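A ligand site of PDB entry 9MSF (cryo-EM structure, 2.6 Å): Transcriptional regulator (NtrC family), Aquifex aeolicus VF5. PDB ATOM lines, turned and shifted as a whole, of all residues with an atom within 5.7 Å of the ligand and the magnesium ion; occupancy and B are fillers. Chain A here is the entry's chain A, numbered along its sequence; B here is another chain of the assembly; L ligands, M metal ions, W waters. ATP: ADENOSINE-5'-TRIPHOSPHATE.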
ATOM      1  N   GLU A  19      18.091 -10.893 -20.029  1.00  0.00           N
ATOM      2  CA  GLU A  19      17.523  -9.929 -19.096  1.00  0.00           C
ATOM      3  C   GLU A  19      16.589 -10.625 -18.103  1.00  0.00           C
ATOM      4  O   GLU A  19      15.900 -11.584 -18.454  1.00  0.00           O
ATOM      5  CB  GLU A  19      16.761  -8.840 -19.848  1.00  0.00           C
ATOM      6  CG  GLU A  19      16.226  -7.723 -18.965  1.00  0.00           C
ATOM      7  CD  GLU A  19      15.374  -6.734 -19.728  1.00  0.00           C
ATOM      8  OE1 GLU A  19      15.340  -6.808 -20.974  1.00  0.00           O
ATOM      9  OE2 GLU A  19      14.734  -5.875 -19.075  1.00  0.00           O
ATOM     10  N   TYR A  20      16.582 -10.135 -16.866  1.00  0.00           N
ATOM     11  CA  TYR A  20      15.772 -10.697 -15.796  1.00  0.00           C
ATOM     12  C   TYR A  20      14.853  -9.624 -15.235  1.00  0.00           C
ATOM     13  O   TYR A  20      15.021  -8.420 -15.505  1.00  0.00           O
ATOM     14  CB  TYR A  20      16.652 -11.292 -14.693  1.00  0.00           C
ATOM     15  CG  TYR A  20      17.500 -12.455 -15.154  1.00  0.00           C
ATOM     16  CD1 TYR A  20      16.971 -13.416 -16.013  1.00  0.00           C
ATOM     17  CD2 TYR A  20      18.813 -12.581 -14.743  1.00  0.00           C
ATOM     18  CE1 TYR A  20      17.742 -14.476 -16.439  1.00  0.00           C
ATOM     19  CE2 TYR A  20      19.591 -13.648 -15.171  1.00  0.00           C
ATOM     20  CZ  TYR A  20      19.052 -14.592 -16.018  1.00  0.00           C
ATOM     21  OH  TYR A  20      19.816 -15.647 -16.441  1.00  0.00           O
ATOM     22  N   VAL A  21      13.873 -10.054 -14.452  1.00  0.00           N
ATOM     23  CA  VAL A  21      12.844  -9.168 -13.903  1.00  0.00           C
ATOM     24  C   VAL A  21      12.971  -9.152 -12.387  1.00  0.00           C
ATOM     25  O   VAL A  21      12.891 -10.206 -11.739  1.00  0.00           O
ATOM     26  CB  VAL A  21      11.426  -9.620 -14.329  1.00  0.00           C
ATOM     27  CG1 VAL A  21      10.385  -8.745 -13.663  1.00  0.00           C
ATOM     28  CG2 VAL A  21      11.290  -9.570 -15.840  1.00  0.00           C
ATOM     29  N   PHE A  22      13.157  -7.956 -11.829  1.00  0.00           N
ATOM     30  CA  PHE A  22      13.192  -7.738 -10.375  1.00  0.00           C
ATOM     31  C   PHE A  22      12.358  -6.485 -10.105  1.00  0.00           C
ATOM     32  O   PHE A  22      12.886  -5.368 -10.122  1.00  0.00           O
ATOM     33  CB  PHE A  22      14.616  -7.599  -9.859  1.00  0.00           C
ATOM     34  CG  PHE A  22      15.509  -8.761 -10.184  1.00  0.00           C
ATOM     35  CD1 PHE A  22      15.478  -9.910  -9.426  1.00  0.00           C
ATOM     36  CD2 PHE A  22      16.393  -8.683 -11.252  1.00  0.00           C
ATOM     37  CE1 PHE A  22      16.297 -10.979  -9.726  1.00  0.00           C
ATOM     38  CE2 PHE A  22      17.216  -9.745 -11.558  1.00  0.00           C
ATOM     39  CZ  PHE A  22      17.174 -10.894 -10.792  1.00  0.00           C
ATOM     40  N   GLY A  48      15.776 -21.690  -1.062  1.00  0.00           N
ATOM     41  CA  GLY A  48      14.483 -21.258  -1.553  1.00  0.00           C
ATOM     42  C   GLY A  48      13.665 -22.453  -1.972  1.00  0.00           C
ATOM     43  O   GLY A  48      14.080 -23.601  -1.844  1.00  0.00           O
ATOM     44  N   GLU A  49      12.468 -22.153  -2.485  1.00  0.00           N
ATOM     45  CA  GLU A  49      11.570 -23.192  -2.979  1.00  0.00           C
ATOM     46  C   GLU A  49      12.035 -23.609  -4.371  1.00  0.00           C
ATOM     47  O   GLU A  49      13.107 -23.204  -4.846  1.00  0.00           O
ATOM     48  CB  GLU A  49      10.133 -22.698  -2.947  1.00  0.00           C
ATOM     49  CG  GLU A  49       9.107 -23.788  -2.700  1.00  0.00           C
ATOM     50  CD  GLU A  49       7.721 -23.229  -2.434  1.00  0.00           C
ATOM     51  OE1 GLU A  49       7.603 -22.000  -2.273  1.00  0.00           O
ATOM     52  OE2 GLU A  49       6.757 -24.010  -2.388  1.00  0.00           O
ATOM     53  N   SER A  50      11.246 -24.431  -5.059  1.00  0.00           N
ATOM     54  CA  SER A  50      11.610 -24.914  -6.379  1.00  0.00           C
ATOM     55  C   SER A  50      11.271 -23.865  -7.431  1.00  0.00           C
ATOM     56  O   SER A  50      10.174 -23.305  -7.442  1.00  0.00           O
ATOM     57  CB  SER A  50      10.883 -26.223  -6.682  1.00  0.00           C
ATOM     58  OG  SER A  50      11.293 -26.739  -7.942  1.00  0.00           O
ATOM     59  N   GLY A  51      12.233 -23.592  -8.314  1.00  0.00           N
ATOM     60  CA  GLY A  51      12.024 -22.647  -9.398  1.00  0.00           C
ATOM     61  C   GLY A  51      11.839 -21.206  -8.960  1.00  0.00           C
ATOM     62  O   GLY A  51      10.995 -20.502  -9.530  1.00  0.00           O
ATOM     63  N   VAL A  52      12.611 -20.750  -7.988  1.00  0.00           N
ATOM     64  CA  VAL A  52      12.481 -19.382  -7.479  1.00  0.00           C
ATOM     65  C   VAL A  52      13.516 -18.472  -8.144  1.00  0.00           C
ATOM     66  O   VAL A  52      13.307 -17.266  -8.246  1.00  0.00           O
ATOM     67  CB  VAL A  52      12.621 -19.342  -5.944  1.00  0.00           C
ATOM     68  CG1 VAL A  52      11.370 -19.897  -5.294  1.00  0.00           C
ATOM     69  CG2 VAL A  52      13.841 -20.123  -5.511  1.00  0.00           C
ATOM     70  N   GLY A  53      14.621 -19.047  -8.609  1.00  0.00           N
ATOM     71  CA  GLY A  53      15.643 -18.255  -9.253  1.00  0.00           C
ATOM     72  C   GLY A  53      17.020 -18.355  -8.628  1.00  0.00           C
ATOM     73  O   GLY A  53      17.821 -17.421  -8.742  1.00  0.00           O
ATOM     74  N   LYS A  54      17.313 -19.475  -7.951  1.00  0.00           N
ATOM     75  CA  LYS A  54      18.599 -19.633  -7.289  1.00  0.00           C
ATOM     76  C   LYS A  54      19.754 -19.612  -8.288  1.00  0.00           C
ATOM     77  O   LYS A  54      20.807 -19.020  -8.018  1.00  0.00           O
ATOM     78  CB  LYS A  54      18.603 -20.922  -6.470  1.00  0.00           C
ATOM     79  CG  LYS A  54      17.645 -20.903  -5.302  1.00  0.00           C
ATOM     80  CD  LYS A  54      17.619 -22.250  -4.592  1.00  0.00           C
ATOM     81  CE  LYS A  54      17.012 -23.310  -5.471  1.00  0.00           C
ATOM     82  NZ  LYS A  54      16.954 -24.624  -4.779  1.00  0.00           N
ATOM     83  N   GLU A  55      19.577 -20.269  -9.443  1.00  0.00           N
ATOM     84  CA  GLU A  55      20.599 -20.216 -10.480  1.00  0.00           C
ATOM     85  C   GLU A  55      20.790 -18.788 -10.978  1.00  0.00           C
ATOM     86  O   GLU A  55      21.919 -18.351 -11.235  1.00  0.00           O
ATOM     87  CB  GLU A  55      20.225 -21.138 -11.630  1.00  0.00           C
ATOM     88  CG  GLU A  55      21.251 -21.210 -12.745  1.00  0.00           C
ATOM     89  CD  GLU A  55      22.333 -22.222 -12.466  1.00  0.00           C
ATOM     90  OE1 GLU A  55      22.198 -22.988 -11.492  1.00  0.00           O
ATOM     91  OE2 GLU A  55      23.325 -22.262 -13.223  1.00  0.00           O
ATOM     92  N   VAL A  56      19.689 -18.054 -11.125  1.00  0.00           N
ATOM     93  CA  VAL A  56      19.764 -16.654 -11.531  1.00  0.00           C
ATOM     94  C   VAL A  56      20.573 -15.850 -10.527  1.00  0.00           C
ATOM     95  O   VAL A  56      21.434 -15.050 -10.896  1.00  0.00           O
ATOM     96  CB  VAL A  56      18.343 -16.076 -11.713  1.00  0.00           C
ATOM     97  CG1 VAL A  56      18.410 -14.566 -11.890  1.00  0.00           C
ATOM     98  CG2 VAL A  56      17.660 -16.729 -12.894  1.00  0.00           C
ATOM     99  N   ASP A 119      25.032 -27.251  -6.946  1.00  0.00           N
ATOM    100  CA  ASP A 119      23.575 -27.225  -6.996  1.00  0.00           C
ATOM    101  C   ASP A 119      23.023 -28.400  -6.190  1.00  0.00           C
ATOM    102  O   ASP A 119      23.515 -29.525  -6.306  1.00  0.00           O
ATOM    103  CB  ASP A 119      23.086 -27.282  -8.437  1.00  0.00           C
ATOM    104  CG  ASP A 119      21.724 -26.651  -8.618  1.00  0.00           C
ATOM    105  OD1 ASP A 119      20.972 -26.548  -7.616  1.00  0.00           O
ATOM    106  OD2 ASP A 119      21.395 -26.253  -9.759  1.00  0.00           O
ATOM    107  N   GLU A 120      22.000 -28.129  -5.382  1.00  0.00           N
ATOM    108  CA  GLU A 120      21.360 -29.125  -4.526  1.00  0.00           C
ATOM    109  C   GLU A 120      22.384 -29.773  -3.591  1.00  0.00           C
ATOM    110  O   GLU A 120      22.664 -30.974  -3.656  1.00  0.00           O
ATOM    111  CB  GLU A 120      20.621 -30.178  -5.370  1.00  0.00           C
ATOM    112  CG  GLU A 120      19.657 -31.048  -4.590  1.00  0.00           C
ATOM    113  CD  GLU A 120      18.516 -30.256  -3.975  1.00  0.00           C
ATOM    114  OE1 GLU A 120      18.126 -29.213  -4.538  1.00  0.00           O
ATOM    115  OE2 GLU A 120      18.007 -30.685  -2.911  1.00  0.00           O
ATOM    116  N   ASN A 161      17.259 -26.490  -1.937  1.00  0.00           N
ATOM    117  CA  ASN A 161      15.851 -26.238  -1.680  1.00  0.00           C
ATOM    118  C   ASN A 161      15.327 -26.957  -0.444  1.00  0.00           C
ATOM    119  O   ASN A 161      14.170 -26.745  -0.058  1.00  0.00           O
ATOM    120  CB  ASN A 161      14.995 -26.620  -2.896  1.00  0.00           C
ATOM    121  CG  ASN A 161      15.234 -28.038  -3.355  1.00  0.00           C
ATOM    122  OD1 ASN A 161      15.883 -28.837  -2.676  1.00  0.00           O
ATOM    123  ND2 ASN A 161      14.713 -28.378  -4.525  1.00  0.00           N
ATOM    124  N   ARG A 194       5.060 -12.909  -4.268  1.00  0.00           N
ATOM    125  CA  ARG A 194       5.591 -11.908  -5.178  1.00  0.00           C
ATOM    126  C   ARG A 194       4.557 -11.558  -6.238  1.00  0.00           C
ATOM    127  O   ARG A 194       4.877 -11.539  -7.432  1.00  0.00           O
ATOM    128  CB  ARG A 194       6.885 -12.400  -5.821  1.00  0.00           C
ATOM    129  CG  ARG A 194       8.021 -12.617  -4.838  1.00  0.00           C
ATOM    130  CD  ARG A 194       8.953 -13.730  -5.300  1.00  0.00           C
ATOM    131  NE  ARG A 194       9.520 -13.471  -6.614  1.00  0.00           N
ATOM    132  CZ  ARG A 194      10.319 -14.303  -7.260  1.00  0.00           C
ATOM    133  NH1 ARG A 194      10.667 -15.473  -6.742  1.00  0.00           N
ATOM    134  NH2 ARG A 194      10.793 -13.961  -8.454  1.00  0.00           N
ATOM    135  N   ASP A 197       5.052  -9.121  -8.910  1.00  0.00           N
ATOM    136  CA  ASP A 197       6.065  -9.539  -9.867  1.00  0.00           C
ATOM    137  C   ASP A 197       5.542 -10.524 -10.889  1.00  0.00           C
ATOM    138  O   ASP A 197       6.283 -10.893 -11.808  1.00  0.00           O
ATOM    139  CB  ASP A 197       7.257 -10.140  -9.118  1.00  0.00           C
ATOM    140  CG  ASP A 197       8.541 -10.090  -9.923  1.00  0.00           C
ATOM    141  OD1 ASP A 197       8.552  -9.463 -10.996  1.00  0.00           O
ATOM    142  OD2 ASP A 197       9.556 -10.677  -9.470  1.00  0.00           O
ATOM    143  N   LEU A 201       6.547 -10.650 -15.224  1.00  0.00           N
ATOM    144  CA  LEU A 201       7.195 -11.889 -15.643  1.00  0.00           C
ATOM    145  C   LEU A 201       6.480 -12.510 -16.841  1.00  0.00           C
ATOM    146  O   LEU A 201       7.121 -12.871 -17.838  1.00  0.00           O
ATOM    147  CB  LEU A 201       7.244 -12.876 -14.481  1.00  0.00           C
ATOM    148  CG  LEU A 201       8.480 -12.830 -13.590  1.00  0.00           C
ATOM    149  CD1 LEU A 201       8.374 -13.842 -12.465  1.00  0.00           C
ATOM    150  CD2 LEU A 201       9.723 -13.078 -14.405  1.00  0.00           C
ATOM    151  N   HIS A 204       7.033 -10.859 -19.938  1.00  0.00           N
ATOM    152  CA  HIS A 204       8.397 -11.148 -20.356  1.00  0.00           C
ATOM    153  C   HIS A 204       8.465 -12.460 -21.117  1.00  0.00           C
ATOM    154  O   HIS A 204       9.135 -12.549 -22.159  1.00  0.00           O
ATOM    155  CB  HIS A 204       9.325 -11.190 -19.137  1.00  0.00           C
ATOM    156  CG  HIS A 204      10.716 -11.648 -19.449  1.00  0.00           C
ATOM    157  ND1 HIS A 204      11.184 -12.894 -19.110  1.00  0.00           N
ATOM    158  CD2 HIS A 204      11.733 -11.010 -20.076  1.00  0.00           C
ATOM    159  CE1 HIS A 204      12.442 -13.011 -19.516  1.00  0.00           C
ATOM    160  NE2 HIS A 204      12.797 -11.881 -20.102  1.00  0.00           N
ATOM    161  N   PHE A 205       7.777 -13.497 -20.636  1.00  0.00           N
ATOM    162  CA  PHE A 205       7.833 -14.797 -21.303  1.00  0.00           C
ATOM    163  C   PHE A 205       7.004 -14.805 -22.583  1.00  0.00           C
ATOM    164  O   PHE A 205       7.439 -15.372 -23.594  1.00  0.00           O
ATOM    165  CB  PHE A 205       7.363 -15.899 -20.353  1.00  0.00           C
ATOM    166  CG  PHE A 205       8.344 -16.199 -19.253  1.00  0.00           C
ATOM    167  CD1 PHE A 205       9.565 -16.768 -19.543  1.00  0.00           C
ATOM    168  CD2 PHE A 205       8.034 -15.921 -17.935  1.00  0.00           C
ATOM    169  CE1 PHE A 205      10.463 -17.053 -18.533  1.00  0.00           C
ATOM    170  CE2 PHE A 205       8.924 -16.199 -16.923  1.00  0.00           C
ATOM    171  CZ  PHE A 205      10.140 -16.771 -17.220  1.00  0.00           C
ATOM    172  N   LYS A 208       8.971 -13.698 -25.443  1.00  0.00           N
ATOM    173  CA  LYS A 208      10.121 -14.522 -25.781  1.00  0.00           C
ATOM    174  C   LYS A 208       9.718 -15.757 -26.572  1.00  0.00           C
ATOM    175  O   LYS A 208      10.390 -16.141 -27.541  1.00  0.00           O
ATOM    176  CB  LYS A 208      10.876 -14.927 -24.519  1.00  0.00           C
ATOM    177  CG  LYS A 208      12.116 -15.769 -24.782  1.00  0.00           C
ATOM    178  CD  LYS A 208      12.857 -16.088 -23.495  1.00  0.00           C
ATOM    179  CE  LYS A 208      12.000 -16.913 -22.551  1.00  0.00           C
ATOM    180  NZ  LYS A 208      12.746 -17.257 -21.308  1.00  0.00           N
ATOM    181  N   VAL A 237       8.396 -19.834 -10.741  1.00  0.00           N
ATOM    182  CA  VAL A 237       8.598 -19.213 -12.047  1.00  0.00           C
ATOM    183  C   VAL A 237       8.625 -20.246 -13.169  1.00  0.00           C
ATOM    184  O   VAL A 237       8.160 -19.971 -14.280  1.00  0.00           O
ATOM    185  CB  VAL A 237       9.884 -18.359 -12.037  1.00  0.00           C
ATOM    186  CG1 VAL A 237       9.985 -17.536 -13.309  1.00  0.00           C
ATOM    187  CG2 VAL A 237       9.913 -17.474 -10.813  1.00  0.00           C
ATOM    188  N   ARG A 238       9.162 -21.443 -12.912  1.00  0.00           N
ATOM    189  CA  ARG A 238       9.234 -22.453 -13.958  1.00  0.00           C
ATOM    190  C   ARG A 238       7.844 -22.901 -14.392  1.00  0.00           C
ATOM    191  O   ARG A 238       7.593 -23.105 -15.587  1.00  0.00           O
ATOM    192  CB  ARG A 238      10.061 -23.645 -13.490  1.00  0.00           C
ATOM    193  CG  ARG A 238      10.223 -24.715 -14.561  1.00  0.00           C
ATOM    194  CD  ARG A 238      11.031 -25.901 -14.083  1.00  0.00           C
ATOM    195  NE  ARG A 238      12.447 -25.597 -13.940  1.00  0.00           N
ATOM    196  CZ  ARG A 238      13.097 -25.576 -12.788  1.00  0.00           C
ATOM    197  NH1 ARG A 238      12.491 -25.845 -11.650  1.00  0.00           N
ATOM    198  NH2 ARG A 238      14.397 -25.276 -12.782  1.00  0.00           N
ATOM    199  N   LYS A 241       6.424 -20.246 -16.570  1.00  0.00           N
ATOM    200  CA  LYS A 241       7.036 -20.325 -17.899  1.00  0.00           C
ATOM    201  C   LYS A 241       6.421 -21.447 -18.721  1.00  0.00           C
ATOM    202  O   LYS A 241       6.132 -21.269 -19.911  1.00  0.00           O
ATOM    203  CB  LYS A 241       8.541 -20.518 -17.760  1.00  0.00           C
ATOM    204  CG  LYS A 241       9.303 -20.525 -19.068  1.00  0.00           C
ATOM    205  CD  LYS A 241      10.773 -20.815 -18.864  1.00  0.00           C
ATOM    206  CE  LYS A 241      10.969 -22.178 -18.222  1.00  0.00           C
ATOM    207  NZ  LYS A 241      12.404 -22.493 -18.021  1.00  0.00           N
ATOM    208  N   ARG B 134      19.929 -31.527 -14.052  1.00  0.00           N
ATOM    209  CA  ARG B 134      20.577 -30.477 -14.819  1.00  0.00           C
ATOM    210  C   ARG B 134      20.666 -30.772 -16.313  1.00  0.00           C
ATOM    211  O   ARG B 134      20.698 -29.829 -17.111  1.00  0.00           O
ATOM    212  CB  ARG B 134      21.990 -30.215 -14.283  1.00  0.00           C
ATOM    213  CG  ARG B 134      22.023 -29.554 -12.914  1.00  0.00           C
ATOM    214  CD  ARG B 134      23.414 -29.050 -12.582  1.00  0.00           C
ATOM    215  NE  ARG B 134      23.888 -28.064 -13.550  1.00  0.00           N
ATOM    216  CZ  ARG B 134      23.684 -26.757 -13.441  1.00  0.00           C
ATOM    217  NH1 ARG B 134      23.014 -26.247 -12.424  1.00  0.00           N
ATOM    218  NH2 ARG B 134      24.148 -25.949 -14.389  1.00  0.00           N
ATOM    219  N   GLU B 137      17.303 -29.748 -18.063  1.00  0.00           N
ATOM    220  CA  GLU B 137      17.114 -28.307 -18.176  1.00  0.00           C
ATOM    221  C   GLU B 137      17.997 -27.701 -19.263  1.00  0.00           C
ATOM    222  O   GLU B 137      17.489 -27.106 -20.224  1.00  0.00           O
ATOM    223  CB  GLU B 137      17.397 -27.649 -16.824  1.00  0.00           C
ATOM    224  CG  GLU B 137      16.173 -27.353 -15.991  1.00  0.00           C
ATOM    225  CD  GLU B 137      15.539 -26.008 -16.309  1.00  0.00           C
ATOM    226  OE1 GLU B 137      15.847 -25.459 -17.388  1.00  0.00           O
ATOM    227  OE2 GLU B 137      14.746 -25.504 -15.488  1.00  0.00           O
ATOM    228  N   ASP B 176      10.797 -31.338  -8.388  1.00  0.00           N
ATOM    229  CA  ASP B 176      11.555 -30.571  -9.368  1.00  0.00           C
ATOM    230  C   ASP B 176      11.581 -31.280 -10.718  1.00  0.00           C
ATOM    231  O   ASP B 176      11.422 -30.637 -11.772  1.00  0.00           O
ATOM    232  CB  ASP B 176      12.978 -30.331  -8.868  1.00  0.00           C
ATOM    233  CG  ASP B 176      13.171 -30.777  -7.433  1.00  0.00           C
ATOM    234  OD1 ASP B 176      12.204 -30.716  -6.650  1.00  0.00           O
ATOM    235  OD2 ASP B 176      14.299 -31.205  -7.087  1.00  0.00           O
ATOM    236  N   ARG B 180      10.301 -30.103 -14.422  1.00  0.00           N
ATOM    237  CA  ARG B 180      11.275 -30.104 -15.505  1.00  0.00           C
ATOM    238  C   ARG B 180      10.775 -30.882 -16.708  1.00  0.00           C
ATOM    239  O   ARG B 180      10.964 -30.463 -17.855  1.00  0.00           O
ATOM    240  CB  ARG B 180      12.606 -30.669 -15.010  1.00  0.00           C
ATOM    241  CG  ARG B 180      13.458 -29.676 -14.245  1.00  0.00           C
ATOM    242  CD  ARG B 180      14.717 -30.334 -13.723  1.00  0.00           C
ATOM    243  NE  ARG B 180      15.728 -29.357 -13.345  1.00  0.00           N
ATOM    244  CZ  ARG B 180      15.791 -28.766 -12.160  1.00  0.00           C
ATOM    245  NH1 ARG B 180      14.912 -29.030 -11.209  1.00  0.00           N
ATOM    246  NH2 ARG B 180      16.764 -27.892 -11.917  1.00  0.00           N
HETATM  247  PG  ATP L   1      15.381 -25.972  -8.501  1.00  0.00           P
HETATM  248  O1G ATP L   1      16.676 -26.648  -8.783  1.00  0.00           O
HETATM  249  O2G ATP L   1      15.204 -25.583  -7.026  1.00  0.00           O
HETATM  250  O3G ATP L   1      14.155 -26.755  -8.969  1.00  0.00           O
HETATM  251  PB  ATP L   1      16.026 -23.183  -9.341  1.00  0.00           P
HETATM  252  O1B ATP L   1      15.530 -22.257  -8.300  1.00  0.00           O
HETATM  253  O2B ATP L   1      17.526 -23.467  -9.314  1.00  0.00           O
HETATM  254  O3B ATP L   1      15.295 -24.587  -9.279  1.00  0.00           O
HETATM  255  PA  ATP L   1      16.197 -21.600 -11.810  1.00  0.00           P
HETATM  256  O1A ATP L   1      16.982 -22.200 -12.906  1.00  0.00           O
HETATM  257  O2A ATP L   1      16.960 -20.576 -10.984  1.00  0.00           O
HETATM  258  O3A ATP L   1      15.660 -22.690 -10.806  1.00  0.00           O
HETATM  259  O5' ATP L   1      14.866 -20.915 -12.332  1.00  0.00           O
HETATM  260  C5' ATP L   1      13.958 -21.613 -13.210  1.00  0.00           C
HETATM  261  C4' ATP L   1      13.645 -20.687 -14.357  1.00  0.00           C
HETATM  262  O4' ATP L   1      13.214 -19.421 -13.840  1.00  0.00           O
HETATM  263  C3' ATP L   1      14.827 -20.420 -15.298  1.00  0.00           C
HETATM  264  O3' ATP L   1      14.584 -20.942 -16.595  1.00  0.00           O
HETATM  265  C2' ATP L   1      14.969 -18.885 -15.306  1.00  0.00           C
HETATM  266  O2' ATP L   1      15.141 -18.388 -16.629  1.00  0.00           O
HETATM  267  C1' ATP L   1      13.624 -18.410 -14.736  1.00  0.00           C
HETATM  268  N9  ATP L   1      13.713 -17.160 -13.993  1.00  0.00           N
HETATM  269  C8  ATP L   1      13.951 -17.011 -12.650  1.00  0.00           C
HETATM  270  N7  ATP L   1      13.954 -15.764 -12.245  1.00  0.00           N
HETATM  271  C5  ATP L   1      13.708 -15.042 -13.402  1.00  0.00           C
HETATM  272  C6  ATP L   1      13.590 -13.661 -13.641  1.00  0.00           C
HETATM  273  N6  ATP L   1      13.718 -12.726 -12.700  1.00  0.00           N
HETATM  274  N1  ATP L   1      13.337 -13.270 -14.909  1.00  0.00           N
HETATM  275  C2  ATP L   1      13.207 -14.201 -15.864  1.00  0.00           C
HETATM  276  N3  ATP L   1      13.292 -15.529 -15.740  1.00  0.00           N
HETATM  277  C4  ATP L   1      13.548 -15.884 -14.477  1.00  0.00           C
HETATM  278 MG    MG M   1      18.637 -25.472  -9.505  1.00  0.00          MG
HETATM  279  O   HOH W   1      13.997 -14.800  -9.184  1.00  0.00           O
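The magnesium ion is bound by O2B of the ligand (2.3 Å) and O1G of the ligand (2.4 Å). The magnesium ion has two donor atoms within binding distance.
Water W1 lies within hydrogen-bond range of the backbone carbonyl oxygen of Val 52, a nitrogen (N7) of the ligand and the guanidinium group of Arg 194.
NZ of Lys 54 lies within salt-bridge range of O2G of the ligand, at 3.0 Å. The guanidinium group (NH1) of Arg 180 of chain B lies within salt-bridge range of an oxygen (O3G) of the ligand (3.3 Å). The backbone NH (N) of Val 21 lies within hydrogen-bond range of a nitrogen (N1) of the ligand (3.3 Å). The side-chain amino group of Lys 241 sits at hydrogen-bond distance from an oxygen (O3') of the ligand (3.0 Å). An oxygen (O3G) of the ligand is in salt-bridge range of the guanidinium group of Arg 238. O2A of the ligand sits at hydrogen-bond distance from N of Glu 55, 3.1 Å away. O3B of the ligand is in hydrogen-bond range of N of Gly 51 (3.4 Å). N of Gly 53 sits at hydrogen-bond distance from O1B of the ligand (3.4 Å). A nitrogen (N6) of the ligand is in hydrogen-bond range of the backbone carbonyl oxygen of Val 21, 2.8 Å away. N of Val 52 lies within hydrogen-bond range of O1B of the ligand (3.3 Å). The side-chain hydroxyl (OG) of Ser 50 sits at hydrogen-bond distance from an oxygen (O3G) of the ligand, 3.0 Å away. N of Lys 54 lies within hydrogen-bond range of O2A of the ligand.
O of Gly 51 is in hydrogen-bond range of N of Val 237, at 2.9 Å. NH1 of Arg 134 of chain B lies within salt-bridge range of OD2 of Asp 119 (3.1 Å). OE1 of Glu 55 is in salt-bridge range of NH1 of Arg 134 of chain B, at 3.5 Å. The guanidinium group of Arg 238 lies within salt-bridge range of the side-chain carboxylate of Glu 137 of chain B. The side-chain carboxylate (OE2) of Glu 120 lies close to the side-chain amide oxygen (OD1) of Asn 161, 2.8 Å away.
CA of Tyr 20 touches N1 of the ligand (3.7 Å). Glu 49 touches the ligand. N of Val 56 touches O2A of the ligand, at 3.7 Å. Asn 161 touches the ligand (ND2 to O2G, 3.8 Å). Leu 201 touches the ligand. His 204 touches the ligand. CZ of Phe 205 touches N3 of the ligand, at 3.7 Å. CG1 of Val 237 touches O4' of the ligand, at 3.8 Å. CB of Asp 176 of chain B touches O3G of the ligand (3.8 Å). Along chain A the residues within 4 Å of the ligand span positions 20 to 241.
Residues that only touch the magnesium ion: Asp 119 (2.9 Å) and Arg 180 of chain B (3.9 Å). The nearest printed residue that does not touch the magnesium ion is Glu 55 (4.8 Å).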
